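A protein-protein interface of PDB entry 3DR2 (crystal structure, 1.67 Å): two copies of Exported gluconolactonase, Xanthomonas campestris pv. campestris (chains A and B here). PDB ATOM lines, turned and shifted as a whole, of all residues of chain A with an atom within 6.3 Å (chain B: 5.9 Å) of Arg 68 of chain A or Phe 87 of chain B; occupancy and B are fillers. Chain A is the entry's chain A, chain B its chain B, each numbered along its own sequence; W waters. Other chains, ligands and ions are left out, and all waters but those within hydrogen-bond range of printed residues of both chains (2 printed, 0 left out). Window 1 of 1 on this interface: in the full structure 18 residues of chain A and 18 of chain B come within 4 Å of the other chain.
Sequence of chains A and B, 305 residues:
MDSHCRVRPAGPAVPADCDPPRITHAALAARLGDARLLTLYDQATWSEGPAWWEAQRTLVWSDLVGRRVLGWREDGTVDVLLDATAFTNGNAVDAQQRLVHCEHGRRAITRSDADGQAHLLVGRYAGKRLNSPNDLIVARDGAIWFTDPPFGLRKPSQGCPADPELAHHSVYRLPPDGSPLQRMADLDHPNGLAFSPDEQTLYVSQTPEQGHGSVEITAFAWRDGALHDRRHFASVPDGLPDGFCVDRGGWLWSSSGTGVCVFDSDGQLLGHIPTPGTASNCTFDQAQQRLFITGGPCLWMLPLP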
ATOM      1  N   CYS A   5      -4.780 -27.169   4.711  1.00  0.00           N
ATOM      2  CA  CYS A   5      -6.011 -26.849   5.414  1.00  0.00           C
ATOM      3  C   CYS A   5      -7.222 -26.700   4.505  1.00  0.00           C
ATOM      4  O   CYS A   5      -7.100 -26.516   3.293  1.00  0.00           O
ATOM      5  CB  CYS A   5      -5.851 -25.595   6.283  1.00  0.00           C
ATOM      6  SG  CYS A   5      -5.846 -23.972   5.455  1.00  0.00           S
ATOM      7  N   VAL A   7     -10.179 -24.637   3.191  1.00  0.00           N
ATOM      8  CA  VAL A   7     -10.543 -23.229   3.088  1.00  0.00           C
ATOM      9  C   VAL A   7     -12.026 -22.973   2.803  1.00  0.00           C
ATOM     10  O   VAL A   7     -12.471 -21.832   2.813  1.00  0.00           O
ATOM     11  CB  VAL A   7      -9.667 -22.496   2.039  1.00  0.00           C
ATOM     12  CG1 VAL A   7      -8.240 -22.361   2.567  1.00  0.00           C
ATOM     13  CG2 VAL A   7      -9.671 -23.256   0.725  1.00  0.00           C
ATOM     14  N   TYR A  41     -16.291 -20.971  -5.197  1.00  0.00           N
ATOM     15  CA  TYR A  41     -15.344 -20.401  -4.247  1.00  0.00           C
ATOM     16  C   TYR A  41     -15.230 -18.919  -4.561  1.00  0.00           C
ATOM     17  O   TYR A  41     -15.280 -18.531  -5.721  1.00  0.00           O
ATOM     18  CB  TYR A  41     -13.971 -21.066  -4.410  1.00  0.00           C
ATOM     19  CG  TYR A  41     -12.978 -20.777  -3.303  1.00  0.00           C
ATOM     20  CD1 TYR A  41     -13.090 -21.397  -2.059  1.00  0.00           C
ATOM     21  CD2 TYR A  41     -11.901 -19.910  -3.512  1.00  0.00           C
ATOM     22  CE1 TYR A  41     -12.155 -21.170  -1.049  1.00  0.00           C
ATOM     23  CE2 TYR A  41     -10.961 -19.673  -2.515  1.00  0.00           C
ATOM     24  CZ  TYR A  41     -11.093 -20.311  -1.281  1.00  0.00           C
ATOM     25  OH  TYR A  41     -10.154 -20.115  -0.292  1.00  0.00           O
ATOM     26  N   TRP A  61      -6.916 -25.729  -9.121  1.00  0.00           N
ATOM     27  CA  TRP A  61      -6.665 -24.426  -9.723  1.00  0.00           C
ATOM     28  C   TRP A  61      -5.767 -23.615  -8.803  1.00  0.00           C
ATOM     29  O   TRP A  61      -5.588 -23.970  -7.640  1.00  0.00           O
ATOM     30  CB  TRP A  61      -7.984 -23.708 -10.052  1.00  0.00           C
ATOM     31  CG  TRP A  61      -8.586 -22.854  -8.990  1.00  0.00           C
ATOM     32  CD1 TRP A  61      -8.545 -21.497  -8.923  1.00  0.00           C
ATOM     33  CD2 TRP A  61      -9.387 -23.288  -7.882  1.00  0.00           C
ATOM     34  NE1 TRP A  61      -9.276 -21.050  -7.848  1.00  0.00           N
ATOM     35  CE2 TRP A  61      -9.805 -22.130  -7.191  1.00  0.00           C
ATOM     36  CE3 TRP A  61      -9.797 -24.543  -7.411  1.00  0.00           C
ATOM     37  CZ2 TRP A  61     -10.611 -22.186  -6.048  1.00  0.00           C
ATOM     38  CZ3 TRP A  61     -10.598 -24.599  -6.274  1.00  0.00           C
ATOM     39  CH2 TRP A  61     -10.996 -23.425  -5.606  1.00  0.00           C
ATOM     40  N   SER A  62      -5.173 -22.549  -9.329  1.00  0.00           N
ATOM     41  CA  SER A  62      -4.255 -21.741  -8.537  1.00  0.00           C
ATOM     42  C   SER A  62      -4.776 -20.404  -8.066  1.00  0.00           C
ATOM     43  O   SER A  62      -5.570 -19.767  -8.740  1.00  0.00           O
ATOM     44  CB  SER A  62      -2.988 -21.427  -9.346  1.00  0.00           C
ATOM     45  OG  SER A  62      -2.341 -22.595  -9.789  1.00  0.00           O
ATOM     46  N   ASP A  63      -4.324 -19.989  -6.889  1.00  0.00           N
ATOM     47  CA  ASP A  63      -4.616 -18.643  -6.427  1.00  0.00           C
ATOM     48  C   ASP A  63      -3.200 -18.094  -6.590  1.00  0.00           C
ATOM     49  O   ASP A  63      -2.375 -18.214  -5.691  1.00  0.00           O
ATOM     50  CB  ASP A  63      -5.023 -18.574  -4.961  1.00  0.00           C
ATOM     51  CG  ASP A  63      -5.254 -17.138  -4.504  1.00  0.00           C
ATOM     52  OD1 ASP A  63      -5.715 -16.922  -3.365  1.00  0.00           O
ATOM     53  OD2 ASP A  63      -4.970 -16.213  -5.299  1.00  0.00           O
ATOM     54  N   LEU A  64      -2.917 -17.536  -7.763  1.00  0.00           N
ATOM     55  CA  LEU A  64      -1.586 -17.021  -8.090  1.00  0.00           C
ATOM     56  C   LEU A  64      -1.018 -16.063  -7.060  1.00  0.00           C
ATOM     57  O   LEU A  64       0.087 -16.254  -6.559  1.00  0.00           O
ATOM     58  CB  LEU A  64      -1.631 -16.324  -9.450  1.00  0.00           C
ATOM     59  CG  LEU A  64      -0.422 -16.349 -10.396  1.00  0.00           C
ATOM     60  CD1 LEU A  64      -0.530 -15.147 -11.314  1.00  0.00           C
ATOM     61  CD2 LEU A  64       0.898 -16.328  -9.653  1.00  0.00           C
ATOM     62  N   VAL A  65      -1.777 -15.024  -6.748  1.00  0.00           N
ATOM     63  CA  VAL A  65      -1.334 -14.021  -5.799  1.00  0.00           C
ATOM     64  C   VAL A  65      -1.308 -14.517  -4.354  1.00  0.00           C
ATOM     65  O   VAL A  65      -0.475 -14.080  -3.558  1.00  0.00           O
ATOM     66  CB  VAL A  65      -2.213 -12.761  -5.944  1.00  0.00           C
ATOM     67  CG1 VAL A  65      -1.875 -11.740  -4.877  1.00  0.00           C
ATOM     68  CG2 VAL A  65      -1.997 -12.164  -7.330  1.00  0.00           C
ATOM     69  N   GLY A  66      -2.212 -15.437  -4.028  1.00  0.00           N
ATOM     70  CA  GLY A  66      -2.271 -15.991  -2.685  1.00  0.00           C
ATOM     71  C   GLY A  66      -1.271 -17.118  -2.480  1.00  0.00           C
ATOM     72  O   GLY A  66      -1.134 -17.649  -1.379  1.00  0.00           O
ATOM     73  N   ARG A  67      -0.587 -17.492  -3.558  1.00  0.00           N
ATOM     74  CA  ARG A  67       0.428 -18.531  -3.521  1.00  0.00           C
ATOM     75  C   ARG A  67      -0.042 -19.878  -2.994  1.00  0.00           C
ATOM     76  O   ARG A  67       0.548 -20.462  -2.084  1.00  0.00           O
ATOM     77  CB  ARG A  67       1.636 -18.017  -2.733  1.00  0.00           C
ATOM     78  CG  ARG A  67       2.083 -16.647  -3.237  1.00  0.00           C
ATOM     79  CD  ARG A  67       3.219 -16.044  -2.425  1.00  0.00           C
ATOM     80  NE  ARG A  67       4.472 -16.774  -2.596  1.00  0.00           N
ATOM     81  CZ  ARG A  67       5.655 -16.323  -2.189  1.00  0.00           C
ATOM     82  NH1 ARG A  67       5.746 -15.142  -1.587  1.00  0.00           N
ATOM     83  NH2 ARG A  67       6.748 -17.053  -2.386  1.00  0.00           N
ATOM     84  N   ARG A  68      -1.113 -20.373  -3.602  1.00  0.00           N
ATOM     85  CA  ARG A  68      -1.679 -21.665  -3.247  1.00  0.00           C
ATOM     86  C   ARG A  68      -2.238 -22.340  -4.481  1.00  0.00           C
ATOM     87  O   ARG A  68      -2.586 -21.677  -5.453  1.00  0.00           O
ATOM     88  CB  ARG A  68      -2.838 -21.497  -2.261  1.00  0.00           C
ATOM     89  CG  ARG A  68      -2.458 -21.252  -0.816  1.00  0.00           C
ATOM     90  CD  ARG A  68      -3.727 -21.036  -0.008  1.00  0.00           C
ATOM     91  NE  ARG A  68      -3.519 -21.151   1.430  1.00  0.00           N
ATOM     92  CZ  ARG A  68      -4.270 -20.531   2.335  1.00  0.00           C
ATOM     93  NH1 ARG A  68      -5.260 -19.751   1.947  1.00  0.00           N
ATOM     94  NH2 ARG A  68      -4.046 -20.708   3.627  1.00  0.00           N
ATOM     95  N   VAL A  69      -2.304 -23.668  -4.432  1.00  0.00           N
ATOM     96  CA  VAL A  69      -2.931 -24.457  -5.481  1.00  0.00           C
ATOM     97  C   VAL A  69      -4.059 -25.107  -4.680  1.00  0.00           C
ATOM     98  O   VAL A  69      -3.799 -25.836  -3.715  1.00  0.00           O
ATOM     99  CB  VAL A  69      -2.011 -25.545  -6.052  1.00  0.00           C
ATOM    100  CG1 VAL A  69      -2.832 -26.509  -6.892  1.00  0.00           C
ATOM    101  CG2 VAL A  69      -0.932 -24.912  -6.924  1.00  0.00           C
ATOM    102  N   LEU A  70      -5.297 -24.813  -5.059  1.00  0.00           N
ATOM    103  CA  LEU A  70      -6.481 -25.311  -4.358  1.00  0.00           C
ATOM    104  C   LEU A  70      -7.144 -26.480  -5.065  1.00  0.00           C
ATOM    105  O   LEU A  70      -6.941 -26.692  -6.259  1.00  0.00           O
ATOM    106  CB  LEU A  70      -7.492 -24.176  -4.216  1.00  0.00           C
ATOM    107  CG  LEU A  70      -6.914 -22.906  -3.585  1.00  0.00           C
ATOM    108  CD1 LEU A  70      -7.887 -21.755  -3.733  1.00  0.00           C
ATOM    109  CD2 LEU A  70      -6.598 -23.175  -2.116  1.00  0.00           C
ATOM    110  N   VAL A  80      -6.446 -26.948   0.464  1.00  0.00           N
ATOM    111  CA  VAL A  80      -5.200 -26.414  -0.064  1.00  0.00           C
ATOM    112  C   VAL A  80      -4.354 -27.635  -0.433  1.00  0.00           C
ATOM    113  O   VAL A  80      -3.987 -28.429   0.442  1.00  0.00           O
ATOM    114  CB  VAL A  80      -4.449 -25.574   0.993  1.00  0.00           C
ATOM    115  CG1 VAL A  80      -3.108 -25.103   0.427  1.00  0.00           C
ATOM    116  CG2 VAL A  80      -5.296 -24.374   1.405  1.00  0.00           C
ATOM    117  N   LEU A  82      -1.407 -27.373  -2.458  1.00  0.00           N
ATOM    118  CA  LEU A  82      -0.018 -26.917  -2.396  1.00  0.00           C
ATOM    119  C   LEU A  82      -0.053 -25.536  -1.753  1.00  0.00           C
ATOM    120  O   LEU A  82      -0.790 -24.665  -2.205  1.00  0.00           O
ATOM    121  CB  LEU A  82       0.592 -26.827  -3.799  1.00  0.00           C
ATOM    122  CG  LEU A  82       0.796 -28.154  -4.529  1.00  0.00           C
ATOM    123  CD1 LEU A  82       1.308 -27.898  -5.934  1.00  0.00           C
ATOM    124  CD2 LEU A  82       1.780 -29.010  -3.759  1.00  0.00           C
ATOM    125  N   ASP A  83       0.739 -25.338  -0.700  1.00  0.00           N
ATOM    126  CA  ASP A  83       0.747 -24.066   0.015  1.00  0.00           C
ATOM    127  C   ASP A  83       2.068 -23.307  -0.121  1.00  0.00           C
ATOM    128  O   ASP A  83       3.119 -23.906  -0.376  1.00  0.00           O
ATOM    129  CB  ASP A  83       0.439 -24.321   1.499  1.00  0.00           C
ATOM    130  CG  ASP A  83       0.001 -23.065   2.236  1.00  0.00           C
ATOM    131  OD1 ASP A  83      -0.826 -22.296   1.691  1.00  0.00           O
ATOM    132  OD2 ASP A  83       0.469 -22.858   3.376  1.00  0.00           O
ATOM    133  N   ALA A  84       1.994 -21.987   0.045  1.00  0.00           N
ATOM    134  CA  ALA A  84       3.159 -21.105  -0.047  1.00  0.00           C
ATOM    135  C   ALA A  84       3.970 -21.401  -1.301  1.00  0.00           C
ATOM    136  O   ALA A  84       5.195 -21.554  -1.254  1.00  0.00           O
ATOM    137  CB  ALA A  84       4.031 -21.265   1.199  1.00  0.00           C
ATOM    138  N   THR A  85       3.276 -21.453  -2.433  1.00  0.00           N
ATOM    139  CA  THR A  85       3.902 -21.760  -3.715  1.00  0.00           C
ATOM    140  C   THR A  85       4.785 -20.642  -4.262  1.00  0.00           C
ATOM    141  O   THR A  85       4.716 -19.493  -3.813  1.00  0.00           O
ATOM    142  CB  THR A  85       2.847 -22.039  -4.771  1.00  0.00           C
ATOM    143  OG1 THR A  85       2.209 -20.806  -5.121  1.00  0.00           O
ATOM    144  CG2 THR A  85       1.798 -23.000  -4.238  1.00  0.00           C
ATOM    145  N   THR A  88       2.623 -20.304  -8.432  1.00  0.00           N
ATOM    146  CA  THR A  88       2.139 -21.264  -9.411  1.00  0.00           C
ATOM    147  C   THR A  88       0.955 -20.661 -10.163  1.00  0.00           C
ATOM    148  O   THR A  88       0.059 -20.067  -9.553  1.00  0.00           O
ATOM    149  CB  THR A  88       1.710 -22.565  -8.717  1.00  0.00           C
ATOM    150  OG1 THR A  88       2.842 -23.127  -8.050  1.00  0.00           O
ATOM    151  CG2 THR A  88       1.184 -23.576  -9.727  1.00  0.00           C
ATOM    152  N   LEU B  64       0.274  -9.015   3.867  1.00  0.00           N
ATOM    153  CA  LEU B  64      -0.417 -10.147   4.462  1.00  0.00           C
ATOM    154  C   LEU B  64      -0.937 -11.153   3.444  1.00  0.00           C
ATOM    155  O   LEU B  64      -0.687 -12.356   3.561  1.00  0.00           O
ATOM    156  CB  LEU B  64      -1.570  -9.632   5.328  1.00  0.00           C
ATOM    157  CG  LEU B  64      -2.510 -10.654   5.965  1.00  0.00           C
ATOM    158  CD1 LEU B  64      -1.737 -11.607   6.848  1.00  0.00           C
ATOM    159  CD2 LEU B  64      -3.568  -9.909   6.779  1.00  0.00           C
ATOM    160  N   VAL B  65      -1.656 -10.664   2.444  1.00  0.00           N
ATOM    161  CA  VAL B  65      -2.232 -11.536   1.428  1.00  0.00           C
ATOM    162  C   VAL B  65      -1.193 -12.139   0.484  1.00  0.00           C
ATOM    163  O   VAL B  65      -1.337 -13.284   0.050  1.00  0.00           O
ATOM    164  CB  VAL B  65      -3.298 -10.772   0.629  1.00  0.00           C
ATOM    165  CG1 VAL B  65      -3.808 -11.613  -0.525  1.00  0.00           C
ATOM    166  CG2 VAL B  65      -4.442 -10.404   1.556  1.00  0.00           C
ATOM    167  N   ARG B  67       1.733 -12.831   1.352  1.00  0.00           N
ATOM    168  CA  ARG B  67       2.600 -13.651   2.190  1.00  0.00           C
ATOM    169  C   ARG B  67       4.075 -13.302   2.117  1.00  0.00           C
ATOM    170  O   ARG B  67       4.922 -14.156   1.865  1.00  0.00           O
ATOM    171  CB  ARG B  67       2.382 -15.118   1.838  1.00  0.00           C
ATOM    172  CG  ARG B  67       0.904 -15.470   1.822  1.00  0.00           C
ATOM    173  CD  ARG B  67       0.652 -16.899   1.394  1.00  0.00           C
ATOM    174  NE  ARG B  67       1.115 -17.857   2.388  1.00  0.00           N
ATOM    175  CZ  ARG B  67       0.786 -19.142   2.380  1.00  0.00           C
ATOM    176  NH1 ARG B  67      -0.007 -19.613   1.426  1.00  0.00           N
ATOM    177  NH2 ARG B  67       1.246 -19.954   3.324  1.00  0.00           N
ATOM    178  N   THR B  85       5.497 -16.369   3.717  1.00  0.00           N
ATOM    179  CA  THR B  85       5.193 -16.367   5.137  1.00  0.00           C
ATOM    180  C   THR B  85       3.877 -17.044   5.456  1.00  0.00           C
ATOM    181  O   THR B  85       3.052 -17.284   4.573  1.00  0.00           O
ATOM    182  CB  THR B  85       5.080 -14.948   5.678  1.00  0.00           C
ATOM    183  OG1 THR B  85       3.918 -14.327   5.118  1.00  0.00           O
ATOM    184  CG2 THR B  85       6.313 -14.144   5.318  1.00  0.00           C
ATOM    185  N   ALA B  86       3.693 -17.334   6.737  1.00  0.00           N
ATOM    186  CA  ALA B  86       2.471 -17.954   7.226  1.00  0.00           C
ATOM    187  C   ALA B  86       1.509 -16.819   7.562  1.00  0.00           C
ATOM    188  O   ALA B  86       1.026 -16.713   8.686  1.00  0.00           O
ATOM    189  CB  ALA B  86       2.761 -18.790   8.477  1.00  0.00           C
ATOM    190  N   PHE B  87       1.262 -15.962   6.577  1.00  0.00           N
ATOM    191  CA  PHE B  87       0.360 -14.826   6.725  1.00  0.00           C
ATOM    192  C   PHE B  87       0.734 -13.892   7.864  1.00  0.00           C
ATOM    193  O   PHE B  87      -0.056 -13.643   8.780  1.00  0.00           O
ATOM    194  CB  PHE B  87      -1.087 -15.312   6.891  1.00  0.00           C
ATOM    195  CG  PHE B  87      -1.565 -16.161   5.748  1.00  0.00           C
ATOM    196  CD1 PHE B  87      -1.469 -17.547   5.806  1.00  0.00           C
ATOM    197  CD2 PHE B  87      -2.062 -15.573   4.589  1.00  0.00           C
ATOM    198  CE1 PHE B  87      -1.856 -18.336   4.727  1.00  0.00           C
ATOM    199  CE2 PHE B  87      -2.452 -16.356   3.500  1.00  0.00           C
ATOM    200  CZ  PHE B  87      -2.348 -17.738   3.573  1.00  0.00           C
ATOM    201  N   THR B  88       1.954 -13.378   7.801  1.00  0.00           N
ATOM    202  CA  THR B  88       2.434 -12.447   8.811  1.00  0.00           C
ATOM    203  C   THR B  88       1.671 -11.139   8.681  1.00  0.00           C
ATOM    204  O   THR B  88       1.507 -10.613   7.579  1.00  0.00           O
ATOM    205  CB  THR B  88       3.922 -12.169   8.628  1.00  0.00           C
ATOM    206  OG1 THR B  88       4.639 -13.404   8.699  1.00  0.00           O
ATOM    207  CG2 THR B  88       4.433 -11.220   9.707  1.00  0.00           C
ATOM    208  N   ASN B  89       1.221 -10.617   9.818  1.00  0.00           N
ATOM    209  CA  ASN B  89       0.461  -9.372   9.862  1.00  0.00           C
ATOM    210  C   ASN B  89       1.315  -8.305  10.552  1.00  0.00           C
ATOM    211  O   ASN B  89       2.189  -7.700   9.921  1.00  0.00           O
ATOM    212  CB  ASN B  89      -0.863  -9.626  10.611  1.00  0.00           C
ATOM    213  CG  ASN B  89      -1.836  -8.459  10.527  1.00  0.00           C
ATOM    214  OD1 ASN B  89      -3.027  -8.614  10.823  1.00  0.00           O
ATOM    215  ND2 ASN B  89      -1.342  -7.289  10.141  1.00  0.00           N
ATOM    216  N   CYS B 102       3.508 -11.148  14.106  1.00  0.00           N
ATOM    217  CA  CYS B 102       2.207 -11.731  14.422  1.00  0.00           C
ATOM    218  C   CYS B 102       1.919 -12.553  13.177  1.00  0.00           C
ATOM    219  O   CYS B 102       1.942 -12.012  12.077  1.00  0.00           O
ATOM    220  CB  CYS B 102       1.125 -10.665  14.546  1.00  0.00           C
ATOM    221  SG  CYS B 102       1.122  -9.803  16.119  1.00  0.00           S
ATOM    222  N   GLU B 103       1.670 -13.850  13.325  1.00  0.00           N
ATOM    223  CA  GLU B 103       1.387 -14.664  12.147  1.00  0.00           C
ATOM    224  C   GLU B 103      -0.004 -15.279  12.203  1.00  0.00           C
ATOM    225  O   GLU B 103      -0.318 -16.037  13.113  1.00  0.00           O
ATOM    226  CB  GLU B 103       2.447 -15.765  11.985  1.00  0.00           C
ATOM    227  CG  GLU B 103       3.847 -15.224  11.679  1.00  0.00           C
ATOM    228  CD  GLU B 103       4.854 -16.323  11.364  1.00  0.00           C
ATOM    229  OE1 GLU B 103       4.424 -17.407  10.940  1.00  0.00           O
ATOM    230  OE2 GLU B 103       6.071 -16.094  11.522  1.00  0.00           O
ATOM    231  N   HIS B 104      -0.842 -14.935  11.233  1.00  0.00           N
ATOM    232  CA  HIS B 104      -2.197 -15.474  11.184  1.00  0.00           C
ATOM    233  C   HIS B 104      -2.176 -16.976  10.953  1.00  0.00           C
ATOM    234  O   HIS B 104      -2.939 -17.721  11.570  1.00  0.00           O
ATOM    235  CB  HIS B 104      -2.997 -14.844  10.043  1.00  0.00           C
ATOM    236  CG  HIS B 104      -3.574 -13.500  10.358  1.00  0.00           C
ATOM    237  ND1 HIS B 104      -4.434 -12.850   9.500  1.00  0.00           N
ATOM    238  CD2 HIS B 104      -3.416 -12.682  11.424  1.00  0.00           C
ATOM    239  CE1 HIS B 104      -4.782 -11.689  10.023  1.00  0.00           C
ATOM    240  NE2 HIS B 104      -4.177 -11.561  11.191  1.00  0.00           N
ATOM    241  N   GLY B 105      -1.307 -17.408  10.045  1.00  0.00           N
ATOM    242  CA  GLY B 105      -1.222 -18.818   9.700  1.00  0.00           C
ATOM    243  C   GLY B 105      -0.816 -19.756  10.815  1.00  0.00           C
ATOM    244  O   GLY B 105      -1.466 -20.780  11.046  1.00  0.00           O
ATOM    245  N   PRO B 156      -9.944 -16.950   4.192  1.00  0.00           N
ATOM    246  CA  PRO B 156      -8.922 -17.779   3.536  1.00  0.00           C
ATOM    247  C   PRO B 156      -7.726 -17.022   2.969  1.00  0.00           C
ATOM    248  O   PRO B 156      -6.601 -17.521   2.991  1.00  0.00           O
ATOM    249  CB  PRO B 156      -9.711 -18.495   2.437  1.00  0.00           C
ATOM    250  CG  PRO B 156     -11.082 -18.601   3.023  1.00  0.00           C
ATOM    251  CD  PRO B 156     -11.279 -17.240   3.639  1.00  0.00           C
ATOM    252  N   SER B 157      -7.964 -15.827   2.447  1.00  0.00           N
ATOM    253  CA  SER B 157      -6.880 -15.037   1.871  1.00  0.00           C
ATOM    254  C   SER B 157      -5.918 -14.535   2.937  1.00  0.00           C
ATOM    255  O   SER B 157      -4.829 -14.021   2.622  1.00  0.00           O
ATOM    256  CB  SER B 157      -7.444 -13.846   1.094  1.00  0.00           C
ATOM    257  OG  SER B 157      -8.252 -13.038   1.929  1.00  0.00           O
ATOM    258  N   GLN B 158      -6.301 -14.707   4.198  1.00  0.00           N
ATOM    259  CA  GLN B 158      -5.476 -14.238   5.304  1.00  0.00           C
ATOM    260  C   GLN B 158      -5.137 -15.277   6.364  1.00  0.00           C
ATOM    261  O   GLN B 158      -4.779 -14.918   7.481  1.00  0.00           O
ATOM    262  CB  GLN B 158      -6.151 -13.032   5.959  1.00  0.00           C
ATOM    263  CG  GLN B 158      -6.399 -11.900   4.980  1.00  0.00           C
ATOM    264  CD  GLN B 158      -6.894 -10.638   5.650  1.00  0.00           C
ATOM    265  OE1 GLN B 158      -6.912 -10.539   6.880  1.00  0.00           O
ATOM    266  NE2 GLN B 158      -7.286  -9.658   4.845  1.00  0.00           N
ATOM    267  N   GLY B 159      -5.247 -16.558   6.020  1.00  0.00           N
ATOM    268  CA  GLY B 159      -4.919 -17.609   6.971  1.00  0.00           C
ATOM    269  C   GLY B 159      -5.634 -18.909   6.669  1.00  0.00           C
ATOM    270  O   GLY B 159      -6.006 -19.157   5.523  1.00  0.00           O
ATOM    271  N   CYS B 160      -5.801 -19.755   7.684  1.00  0.00           N
ATOM    272  CA  CYS B 160      -6.515 -21.020   7.525  1.00  0.00           C
ATOM    273  C   CYS B 160      -7.752 -20.970   8.409  1.00  0.00           C
ATOM    274  O   CYS B 160      -7.648 -20.839   9.633  1.00  0.00           O
ATOM    275  CB  CYS B 160      -5.647 -22.211   7.936  1.00  0.00           C
ATOM    276  SG  CYS B 160      -4.572 -22.888   6.623  1.00  0.00           S
ATOM    277  N   PRO B 161      -8.942 -21.051   7.799  1.00  0.00           N
ATOM    278  CA  PRO B 161     -10.195 -21.009   8.552  1.00  0.00           C
ATOM    279  C   PRO B 161     -10.264 -22.077   9.636  1.00  0.00           C
ATOM    280  O   PRO B 161      -9.752 -23.186   9.469  1.00  0.00           O
ATOM    281  CB  PRO B 161     -11.249 -21.216   7.470  1.00  0.00           C
ATOM    282  CG  PRO B 161     -10.631 -20.569   6.283  1.00  0.00           C
ATOM    283  CD  PRO B 161      -9.206 -21.056   6.348  1.00  0.00           C
HETATM  284  O   HOH W   1      -2.006 -22.136   4.864  1.00  0.00           O
HETATM  285  O   HOH W   2      -8.527 -24.557   7.824  1.00  0.00           O
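The backbone carbonyl oxygen (O) of Pro 156 of chain B is in hydrogen-bond range of the guanidinium group (NH1) of Arg 68 of chain A (2.8 Å).
NH1 of Arg 67 of chain B lies within salt-bridge range of OD1 of Asp 83 of chain A (2.8 Å).
SG of Cys 5 of chain A is disulfide-bonded to SG of Cys 160 of chain B (2.0 Å).
The guanidinium group (NH1) of Arg 67 of chain B lies close to the backbone NH (N) of Ala 84 of chain A.
The guanidinium group of Arg 68 of chain A lies within hydrogen-bond range of the backbone carbonyl oxygen of Gly 159 of chain B (3.1 Å).
NH2 of Arg 68 of chain A is in hydrogen-bond range of SG of Cys 160 of chain B, 3.7 Å away.
Phe 87 of chain B touches just one residue of chain A: Arg 68.
Of the printed residues of chain A, Val 65 of chain B touches Val 65 (3.8 Å) and Gly 66 (3.96 Å).
Of the printed residues of chain B, Val 7 of chain A touches Pro 156 (3.5 Å).
Of the printed residues of chain B, Gly 66 of chain A touches Val 65 (3.96 Å) and Arg 67 (3.4 Å).
Printed residues of chain A within 4 Å of Gly 159 of chain B: Arg 68 (3.1 Å).
Of the printed residues of chain B, Cys 5 of chain A touches Cys 160.
Thr 88 of chain A touches none of the printed residues of chain B.
Thr 85 of chain B touches none of the printed residues of chain A.
The nearest printed residue of chain A that does not touch Phe 87 of chain B is Asp 83 of chain A (5.1 Å).
The nearest printed residue of chain A that does not touch Arg 67 of chain B is Thr 85 of chain A (5.4 Å).
NE of Arg 68 of chain A is in salt-bridge range of OD1 of Asp 83 of chain A (2.9 Å).
The side-chain hydroxyl of Thr 85 of chain B lies close to the backbone NH of Phe 87 of chain B (3.4 Å).
N of Ala 84 of chain A is in hydrogen-bond range of O of Arg 67 of chain A.
The backbone NH (N) of Thr 85 of chain B sits at hydrogen-bond distance from the backbone carbonyl oxygen (O) of Arg 67 of chain B (2.9 Å).
O of Arg 68 of chain A sits at hydrogen-bond distance from N of Asp 63 of chain A.
The backbone NH (N) of Thr 85 of chain A sits at hydrogen-bond distance from the backbone carbonyl oxygen (O) of Arg 67 of chain A (2.9 Å).
CG of Pro 156 of chain B touches O of Val 7 of chain A (3.5 Å).
OH of Tyr 41 of chain A touches CB of Pro 156 of chain B (3.2 Å).
O of Val 65 of chain B touches O of Val 65 of chain A, 3.8 Å away.
Gly 66 of chain A touches Val 65 of chain B.
Gly 66 of chain A touches Arg 67 of chain B (O to CD, 3.4 Å).
Arg 67 of chain B touches Arg 67 of chain A (NH1 to O, 3.7 Å).
Arg 67 of chain B touches Arg 68 of chain A.
NH2 of Arg 68 of chain A touches CE1 of Phe 87 of chain B (3.4 Å).
Water W2 lies within hydrogen-bond range of O of Pro 161 of chain B (2.5 Å) and SG of Cys 5 of chain A (3.6 Å).
Water W1 lies within hydrogen-bond range of the guanidinium group of Arg 68 of chain A, the side-chain carboxylate of Asp 83 of chain A and the side-chain sulfur of Cys 160 of chain B.
Val 65 of chain B touches its own counterpart, Val 65 of chain A.
Arg 67 of chain B touches its own counterpart, Arg 67 of chain A.
Of the 14 pairs that touch across the chains among the printed residues, 2 have their exchanged pair printed and touching as well.
Of the 19 printed residues of chain A, 9 touch a printed residue of chain B.
Printed residues of chain A that touch a printed residue of chain B: Cys 5, Val 7, Tyr 41, Val 65, Gly 66, Arg 67, Arg 68, Asp 83 and Ala 84.
Hydrophobic or aromatic side chains of chain A within 4 Å of the printed part of chain B: Tyr 41 and Ala 84.
Of the 18 printed residues of chain B, 6 touch a printed residue of chain A.
Hydrophobic or aromatic side chains of chain B that line the printed part of chain A: Phe 87 and Pro 156.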
